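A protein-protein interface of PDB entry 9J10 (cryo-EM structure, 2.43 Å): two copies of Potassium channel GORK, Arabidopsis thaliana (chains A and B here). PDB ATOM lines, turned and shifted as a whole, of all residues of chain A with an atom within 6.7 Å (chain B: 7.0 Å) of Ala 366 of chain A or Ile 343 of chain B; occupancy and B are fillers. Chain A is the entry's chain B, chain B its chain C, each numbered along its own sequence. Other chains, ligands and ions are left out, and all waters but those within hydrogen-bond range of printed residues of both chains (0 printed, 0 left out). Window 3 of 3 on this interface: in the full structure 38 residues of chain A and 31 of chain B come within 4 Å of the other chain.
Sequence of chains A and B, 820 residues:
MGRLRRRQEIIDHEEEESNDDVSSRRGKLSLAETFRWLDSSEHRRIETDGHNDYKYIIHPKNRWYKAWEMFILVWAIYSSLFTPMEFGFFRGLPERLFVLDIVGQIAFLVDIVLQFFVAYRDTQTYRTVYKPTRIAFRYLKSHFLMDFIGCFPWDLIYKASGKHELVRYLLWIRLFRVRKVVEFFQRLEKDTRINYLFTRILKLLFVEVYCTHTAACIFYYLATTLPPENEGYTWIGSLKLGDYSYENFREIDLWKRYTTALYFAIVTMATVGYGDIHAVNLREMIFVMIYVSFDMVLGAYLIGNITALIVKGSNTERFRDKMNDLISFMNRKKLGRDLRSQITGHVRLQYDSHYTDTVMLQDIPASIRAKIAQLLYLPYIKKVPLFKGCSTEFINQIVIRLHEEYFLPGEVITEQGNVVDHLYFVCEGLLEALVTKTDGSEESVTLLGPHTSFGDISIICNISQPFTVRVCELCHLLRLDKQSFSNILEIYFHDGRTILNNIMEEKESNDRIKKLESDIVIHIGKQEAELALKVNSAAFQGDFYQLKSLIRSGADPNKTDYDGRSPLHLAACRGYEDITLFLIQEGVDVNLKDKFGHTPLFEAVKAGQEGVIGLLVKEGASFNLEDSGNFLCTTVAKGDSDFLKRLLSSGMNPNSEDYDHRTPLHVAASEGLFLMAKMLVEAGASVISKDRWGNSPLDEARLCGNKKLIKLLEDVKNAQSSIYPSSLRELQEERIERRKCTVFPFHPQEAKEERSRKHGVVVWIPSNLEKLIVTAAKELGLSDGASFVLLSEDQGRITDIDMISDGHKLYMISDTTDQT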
ATOM      1  N   MET A 360      -2.673  33.696  17.617  1.00  0.00           N
ATOM      2  CA  MET A 360      -3.046  32.288  17.632  1.00  0.00           C
ATOM      3  C   MET A 360      -4.236  31.978  16.713  1.00  0.00           C
ATOM      4  O   MET A 360      -5.193  31.326  17.146  1.00  0.00           O
ATOM      5  CB  MET A 360      -3.303  31.841  19.090  1.00  0.00           C
ATOM      6  CG  MET A 360      -3.252  30.320  19.357  1.00  0.00           C
ATOM      7  SD  MET A 360      -1.926  29.517  18.439  1.00  0.00           S
ATOM      8  CE  MET A 360      -2.850  28.208  17.638  1.00  0.00           C
ATOM      9  N   ILE A 364       1.086  28.287  14.802  1.00  0.00           N
ATOM     10  CA  ILE A 364       1.605  26.956  15.102  1.00  0.00           C
ATOM     11  C   ILE A 364       0.397  26.055  15.355  1.00  0.00           C
ATOM     12  O   ILE A 364      -0.608  26.501  15.931  1.00  0.00           O
ATOM     13  CB  ILE A 364       2.635  26.984  16.256  1.00  0.00           C
ATOM     14  CG1 ILE A 364       1.989  26.968  17.648  1.00  0.00           C
ATOM     15  CG2 ILE A 364       3.622  28.157  16.120  1.00  0.00           C
ATOM     16  CD1 ILE A 364       2.983  26.999  18.772  1.00  0.00           C
ATOM     17  N   PRO A 365       0.388  24.820  14.824  1.00  0.00           N
ATOM     18  CA  PRO A 365      -0.755  23.915  14.985  1.00  0.00           C
ATOM     19  C   PRO A 365      -0.757  23.155  16.315  1.00  0.00           C
ATOM     20  O   PRO A 365      -0.355  21.988  16.392  1.00  0.00           O
ATOM     21  CB  PRO A 365      -0.612  22.970  13.789  1.00  0.00           C
ATOM     22  CG  PRO A 365       0.845  22.942  13.514  1.00  0.00           C
ATOM     23  CD  PRO A 365       1.368  24.306  13.850  1.00  0.00           C
ATOM     24  N   ALA A 366      -1.213  23.812  17.373  1.00  0.00           N
ATOM     25  CA  ALA A 366      -1.208  23.213  18.699  1.00  0.00           C
ATOM     26  C   ALA A 366      -2.580  22.660  19.066  1.00  0.00           C
ATOM     27  O   ALA A 366      -3.612  23.217  18.683  1.00  0.00           O
ATOM     28  CB  ALA A 366      -0.767  24.237  19.747  1.00  0.00           C
ATOM     29  N   SER A 367      -2.578  21.556  19.811  1.00  0.00           N
ATOM     30  CA  SER A 367      -3.769  21.040  20.465  1.00  0.00           C
ATOM     31  C   SER A 367      -3.971  21.674  21.835  1.00  0.00           C
ATOM     32  O   SER A 367      -4.996  21.425  22.490  1.00  0.00           O
ATOM     33  CB  SER A 367      -3.682  19.519  20.593  1.00  0.00           C
ATOM     34  OG  SER A 367      -2.622  19.150  21.457  1.00  0.00           O
ATOM     35  N   ILE A 368      -3.012  22.495  22.277  1.00  0.00           N
ATOM     36  CA  ILE A 368      -3.178  23.208  23.536  1.00  0.00           C
ATOM     37  C   ILE A 368      -4.280  24.250  23.418  1.00  0.00           C
ATOM     38  O   ILE A 368      -4.972  24.553  24.400  1.00  0.00           O
ATOM     39  CB  ILE A 368      -1.842  23.830  23.970  1.00  0.00           C
ATOM     40  CG1 ILE A 368      -0.702  22.828  23.786  1.00  0.00           C
ATOM     41  CG2 ILE A 368      -1.887  24.249  25.424  1.00  0.00           C
ATOM     42  CD1 ILE A 368       0.662  23.402  24.064  1.00  0.00           C
ATOM     43  N   ARG A 369      -4.467  24.812  22.215  1.00  0.00           N
ATOM     44  CA  ARG A 369      -5.591  25.714  22.011  1.00  0.00           C
ATOM     45  C   ARG A 369      -6.926  24.983  22.099  1.00  0.00           C
ATOM     46  O   ARG A 369      -7.899  25.567  22.576  1.00  0.00           O
ATOM     47  CB  ARG A 369      -5.468  26.469  20.679  1.00  0.00           C
ATOM     48  CG  ARG A 369      -6.567  27.472  20.339  1.00  0.00           C
ATOM     49  CD  ARG A 369      -6.256  28.126  19.007  1.00  0.00           C
ATOM     50  NE  ARG A 369      -7.298  29.088  18.666  1.00  0.00           N
ATOM     51  CZ  ARG A 369      -8.427  28.785  18.041  1.00  0.00           C
ATOM     52  NH1 ARG A 369      -8.673  27.534  17.677  1.00  0.00           N
ATOM     53  NH2 ARG A 369      -9.310  29.738  17.777  1.00  0.00           N
ATOM     54  N   ALA A 370      -6.978  23.700  21.730  1.00  0.00           N
ATOM     55  CA  ALA A 370      -8.197  22.924  21.940  1.00  0.00           C
ATOM     56  C   ALA A 370      -8.427  22.648  23.420  1.00  0.00           C
ATOM     57  O   ALA A 370      -9.576  22.693  23.886  1.00  0.00           O
ATOM     58  CB  ALA A 370      -8.133  21.608  21.158  1.00  0.00           C
ATOM     59  N   LYS A 371      -7.346  22.397  24.171  1.00  0.00           N
ATOM     60  CA  LYS A 371      -7.469  22.189  25.613  1.00  0.00           C
ATOM     61  C   LYS A 371      -7.975  23.442  26.322  1.00  0.00           C
ATOM     62  O   LYS A 371      -8.953  23.382  27.077  1.00  0.00           O
ATOM     63  CB  LYS A 371      -6.131  21.745  26.204  1.00  0.00           C
ATOM     64  CG  LYS A 371      -5.554  20.474  25.596  1.00  0.00           C
ATOM     65  CD  LYS A 371      -4.072  20.350  25.918  1.00  0.00           C
ATOM     66  CE  LYS A 371      -3.465  19.071  25.363  1.00  0.00           C
ATOM     67  NZ  LYS A 371      -3.170  19.200  23.918  1.00  0.00           N
ATOM     68  N   MET B 323       8.041  35.019  20.008  1.00  0.00           N
ATOM     69  CA  MET B 323       8.062  34.402  21.339  1.00  0.00           C
ATOM     70  C   MET B 323       7.377  35.283  22.380  1.00  0.00           C
ATOM     71  O   MET B 323       6.528  34.818  23.153  1.00  0.00           O
ATOM     72  CB  MET B 323       9.507  34.152  21.779  1.00  0.00           C
ATOM     73  CG  MET B 323      10.313  33.197  20.931  1.00  0.00           C
ATOM     74  SD  MET B 323       9.574  31.572  20.764  1.00  0.00           S
ATOM     75  CE  MET B 323       9.117  31.618  19.038  1.00  0.00           C
ATOM     76  N   ILE B 327       3.819  34.443  24.320  1.00  0.00           N
ATOM     77  CA  ILE B 327       3.751  34.166  25.752  1.00  0.00           C
ATOM     78  C   ILE B 327       3.035  35.298  26.491  1.00  0.00           C
ATOM     79  O   ILE B 327       2.458  35.074  27.564  1.00  0.00           O
ATOM     80  CB  ILE B 327       5.152  33.867  26.328  1.00  0.00           C
ATOM     81  CG1 ILE B 327       5.041  32.963  27.560  1.00  0.00           C
ATOM     82  CG2 ILE B 327       5.911  35.133  26.691  1.00  0.00           C
ATOM     83  CD1 ILE B 327       4.519  31.572  27.263  1.00  0.00           C
ATOM     84  N   MET B 330      -0.484  34.239  26.126  1.00  0.00           N
ATOM     85  CA  MET B 330      -0.714  33.142  27.053  1.00  0.00           C
ATOM     86  C   MET B 330      -0.722  33.583  28.515  1.00  0.00           C
ATOM     87  O   MET B 330      -1.238  32.851  29.364  1.00  0.00           O
ATOM     88  CB  MET B 330       0.337  32.049  26.835  1.00  0.00           C
ATOM     89  CG  MET B 330      -0.118  30.964  25.872  1.00  0.00           C
ATOM     90  SD  MET B 330       1.005  29.560  25.736  1.00  0.00           S
ATOM     91  CE  MET B 330       0.673  29.025  24.056  1.00  0.00           C
ATOM     92  N   ASP B 338       3.039  23.898  32.402  1.00  0.00           N
ATOM     93  CA  ASP B 338       3.833  22.744  31.985  1.00  0.00           C
ATOM     94  C   ASP B 338       3.923  22.601  30.471  1.00  0.00           C
ATOM     95  O   ASP B 338       5.013  22.684  29.894  1.00  0.00           O
ATOM     96  CB  ASP B 338       3.243  21.472  32.586  1.00  0.00           C
ATOM     97  CG  ASP B 338       3.463  21.383  34.072  1.00  0.00           C
ATOM     98  OD1 ASP B 338       4.305  22.144  34.594  1.00  0.00           O
ATOM     99  OD2 ASP B 338       2.797  20.552  34.717  1.00  0.00           O
ATOM    100  N   LEU B 339       2.796  22.395  29.806  1.00  0.00           N
ATOM    101  CA  LEU B 339       2.818  22.089  28.385  1.00  0.00           C
ATOM    102  C   LEU B 339       3.033  23.326  27.525  1.00  0.00           C
ATOM    103  O   LEU B 339       3.439  23.191  26.364  1.00  0.00           O
ATOM    104  CB  LEU B 339       1.531  21.354  27.971  1.00  0.00           C
ATOM    105  CG  LEU B 339       0.169  22.023  27.812  1.00  0.00           C
ATOM    106  CD1 LEU B 339      -0.709  21.070  27.034  1.00  0.00           C
ATOM    107  CD2 LEU B 339      -0.487  22.364  29.145  1.00  0.00           C
ATOM    108  N   ARG B 340       2.835  24.527  28.073  1.00  0.00           N
ATOM    109  CA  ARG B 340       3.263  25.697  27.325  1.00  0.00           C
ATOM    110  C   ARG B 340       4.768  25.914  27.417  1.00  0.00           C
ATOM    111  O   ARG B 340       5.358  26.444  26.474  1.00  0.00           O
ATOM    112  CB  ARG B 340       2.516  26.948  27.785  1.00  0.00           C
ATOM    113  CG  ARG B 340       2.728  27.386  29.221  1.00  0.00           C
ATOM    114  CD  ARG B 340       2.318  28.847  29.353  1.00  0.00           C
ATOM    115  NE  ARG B 340       1.928  29.209  30.715  1.00  0.00           N
ATOM    116  CZ  ARG B 340       1.423  30.390  31.058  1.00  0.00           C
ATOM    117  NH1 ARG B 340       1.228  31.324  30.139  1.00  0.00           N
ATOM    118  NH2 ARG B 340       1.095  30.623  32.321  1.00  0.00           N
ATOM    119  N   SER B 341       5.411  25.483  28.507  1.00  0.00           N
ATOM    120  CA  SER B 341       6.871  25.457  28.529  1.00  0.00           C
ATOM    121  C   SER B 341       7.412  24.409  27.565  1.00  0.00           C
ATOM    122  O   SER B 341       8.451  24.634  26.921  1.00  0.00           O
ATOM    123  CB  SER B 341       7.382  25.208  29.950  1.00  0.00           C
ATOM    124  OG  SER B 341       6.988  23.930  30.415  1.00  0.00           O
ATOM    125  N   GLN B 342       6.709  23.272  27.448  1.00  0.00           N
ATOM    126  CA  GLN B 342       6.956  22.309  26.378  1.00  0.00           C
ATOM    127  C   GLN B 342       6.862  22.934  24.994  1.00  0.00           C
ATOM    128  O   GLN B 342       7.759  22.714  24.175  1.00  0.00           O
ATOM    129  CB  GLN B 342       5.983  21.124  26.489  1.00  0.00           C
ATOM    130  CG  GLN B 342       6.106  20.075  25.366  1.00  0.00           C
ATOM    131  CD  GLN B 342       5.094  20.269  24.240  1.00  0.00           C
ATOM    132  OE1 GLN B 342       3.916  20.531  24.485  1.00  0.00           O
ATOM    133  NE2 GLN B 342       5.564  20.187  23.002  1.00  0.00           N
ATOM    134  N   ILE B 343       5.815  23.714  24.714  1.00  0.00           N
ATOM    135  CA  ILE B 343       5.689  24.229  23.355  1.00  0.00           C
ATOM    136  C   ILE B 343       6.654  25.395  23.119  1.00  0.00           C
ATOM    137  O   ILE B 343       7.053  25.637  21.978  1.00  0.00           O
ATOM    138  CB  ILE B 343       4.226  24.593  23.022  1.00  0.00           C
ATOM    139  CG1 ILE B 343       4.020  24.667  21.506  1.00  0.00           C
ATOM    140  CG2 ILE B 343       3.820  25.921  23.626  1.00  0.00           C
ATOM    141  CD1 ILE B 343       2.725  24.078  21.020  1.00  0.00           C
ATOM    142  N   THR B 344       7.117  26.083  24.175  1.00  0.00           N
ATOM    143  CA  THR B 344       8.156  27.095  23.971  1.00  0.00           C
ATOM    144  C   THR B 344       9.515  26.477  23.664  1.00  0.00           C
ATOM    145  O   THR B 344      10.228  26.981  22.785  1.00  0.00           O
ATOM    146  CB  THR B 344       8.281  28.037  25.174  1.00  0.00           C
ATOM    147  OG1 THR B 344       8.521  27.292  26.373  1.00  0.00           O
ATOM    148  CG2 THR B 344       7.057  28.936  25.311  1.00  0.00           C
ATOM    149  N   GLY B 345       9.894  25.397  24.359  1.00  0.00           N
ATOM    150  CA  GLY B 345      11.072  24.648  23.940  1.00  0.00           C
ATOM    151  C   GLY B 345      10.914  24.044  22.557  1.00  0.00           C
ATOM    152  O   GLY B 345      11.880  23.988  21.777  1.00  0.00           O
ATOM    153  N   HIS B 346       9.685  23.632  22.222  1.00  0.00           N
ATOM    154  CA  HIS B 346       9.371  23.102  20.900  1.00  0.00           C
ATOM    155  C   HIS B 346       9.613  24.136  19.810  1.00  0.00           C
ATOM    156  O   HIS B 346      10.293  23.845  18.826  1.00  0.00           O
ATOM    157  CB  HIS B 346       7.920  22.612  20.877  1.00  0.00           C
ATOM    158  CG  HIS B 346       7.359  22.402  19.504  1.00  0.00           C
ATOM    159  ND1 HIS B 346       6.138  22.915  19.120  1.00  0.00           N
ATOM    160  CD2 HIS B 346       7.823  21.702  18.443  1.00  0.00           C
ATOM    161  CE1 HIS B 346       5.889  22.562  17.872  1.00  0.00           C
ATOM    162  NE2 HIS B 346       6.895  21.825  17.437  1.00  0.00           N
ATOM    163  N   VAL B 347       9.095  25.360  19.980  1.00  0.00           N
ATOM    164  CA  VAL B 347       9.247  26.350  18.915  1.00  0.00           C
ATOM    165  C   VAL B 347      10.676  26.880  18.882  1.00  0.00           C
ATOM    166  O   VAL B 347      11.155  27.298  17.821  1.00  0.00           O
ATOM    167  CB  VAL B 347       8.248  27.520  19.038  1.00  0.00           C
ATOM    168  CG1 VAL B 347       6.847  27.111  18.594  1.00  0.00           C
ATOM    169  CG2 VAL B 347       8.264  28.163  20.407  1.00  0.00           C
ATOM    170  N   ARG B 348      11.381  26.852  20.021  1.00  0.00           N
ATOM    171  CA  ARG B 348      12.787  27.240  20.029  1.00  0.00           C
ATOM    172  C   ARG B 348      13.652  26.268  19.235  1.00  0.00           C
ATOM    173  O   ARG B 348      14.583  26.696  18.542  1.00  0.00           O
ATOM    174  CB  ARG B 348      13.284  27.369  21.471  1.00  0.00           C
ATOM    175  CG  ARG B 348      14.776  27.662  21.639  1.00  0.00           C
ATOM    176  CD  ARG B 348      15.201  29.016  21.064  1.00  0.00           C
ATOM    177  NE  ARG B 348      15.665  28.900  19.681  1.00  0.00           N
ATOM    178  CZ  ARG B 348      16.006  29.925  18.908  1.00  0.00           C
ATOM    179  NH1 ARG B 348      15.954  31.165  19.375  1.00  0.00           N
ATOM    180  NH2 ARG B 348      16.412  29.707  17.665  1.00  0.00           N
ATOM    181  N   LEU B 349      13.349  24.973  19.288  1.00  0.00           N
ATOM    182  CA  LEU B 349      14.069  24.044  18.420  1.00  0.00           C
ATOM    183  C   LEU B 349      13.449  23.906  17.033  1.00  0.00           C
ATOM    184  O   LEU B 349      14.105  23.378  16.126  1.00  0.00           O
ATOM    185  CB  LEU B 349      14.172  22.659  19.067  1.00  0.00           C
ATOM    186  CG  LEU B 349      15.458  22.392  19.860  1.00  0.00           C
ATOM    187  CD1 LEU B 349      16.638  22.476  18.907  1.00  0.00           C
ATOM    188  CD2 LEU B 349      15.648  23.331  21.047  1.00  0.00           C
ATOM    189  N   GLN B 350      12.217  24.373  16.847  1.00  0.00           N
ATOM    190  CA  GLN B 350      11.518  24.291  15.571  1.00  0.00           C
ATOM    191  C   GLN B 350      11.864  25.431  14.625  1.00  0.00           C
ATOM    192  O   GLN B 350      11.939  25.211  13.409  1.00  0.00           O
ATOM    193  CB  GLN B 350      10.005  24.254  15.830  1.00  0.00           C
ATOM    194  CG  GLN B 350       9.102  24.107  14.636  1.00  0.00           C
ATOM    195  CD  GLN B 350       7.903  25.021  14.745  1.00  0.00           C
ATOM    196  OE1 GLN B 350       7.548  25.450  15.838  1.00  0.00           O
ATOM    197  NE2 GLN B 350       7.276  25.328  13.623  1.00  0.00           N
ATOM    198  N   LEU B 408      12.506  17.197  21.036  1.00  0.00           N
ATOM    199  CA  LEU B 408      12.875  17.078  22.439  1.00  0.00           C
ATOM    200  C   LEU B 408      12.560  15.687  22.990  1.00  0.00           C
ATOM    201  O   LEU B 408      11.668  14.997  22.485  1.00  0.00           O
ATOM    202  CB  LEU B 408      12.149  18.137  23.275  1.00  0.00           C
ATOM    203  CG  LEU B 408      10.636  18.069  23.518  1.00  0.00           C
ATOM    204  CD1 LEU B 408      10.295  18.829  24.782  1.00  0.00           C
ATOM    205  CD2 LEU B 408       9.860  18.669  22.357  1.00  0.00           C
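Hydrophobic or aromatic side chains of chain A within 4 Å of the printed part of chain B: Ile 364, Ala 366 and Ile 368.
Printed residues of chain B that touch a printed residue of chain A: Leu 339, Ile 343 and Val 347.
Among the printed residues, 6 pairs touch across the chains.
Among the printed residues, no Asp or Glu carboxylate lies within 4 Å of a Lys or Arg side-chain nitrogen of the other chain.
No position is printed for both chains.
Ala 366 of chain A touches one residue of chain B.
Of the printed residues of chain B, Ile 368 of chain A touches Leu 339 and Ile 343.
Ile 327 of chain B touches none of the printed residues of chain A.
Ser 341 of chain B touches none of the printed residues of chain A.
Of the printed residues of chain A, Val 347 of chain B touches Ile 364.
The nearest residue of chain B that does not touch Ala 366 of chain A is Met 330 of chain B (6.6 Å).
The nearest printed residue of chain B that does not touch Lys 371 of chain A is Gln 342 of chain B (7.2 Å).
The backbone carbonyl oxygen of Leu 339 of chain B sits close to the side-chain amide oxygen of Gln 342 of chain B, 3.3 Å away.
The side-chain hydroxyl (OG) of Ser 367 of chain A lies within hydrogen-bond range of the side-chain amino group (NZ) of Lys 371 of chain A, at 2.5 Å.
Among the printed residues, merely in contact across the chains: Ile 364 of chain A with Ile 343 of chain B (3.7 Å), Ile 364 of chain A with Val 347 of chain B (3.9 Å), Ala 366 of chain A with Ile 343 of chain B (3.7 Å), Ile 368 of chain A with Leu 339 of chain B (3.6 Å), Ile 368 of chain A with Ile 343 of chain B (3.7 Å) and Lys 371 of chain A with Leu 339 of chain B (3.6 Å).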
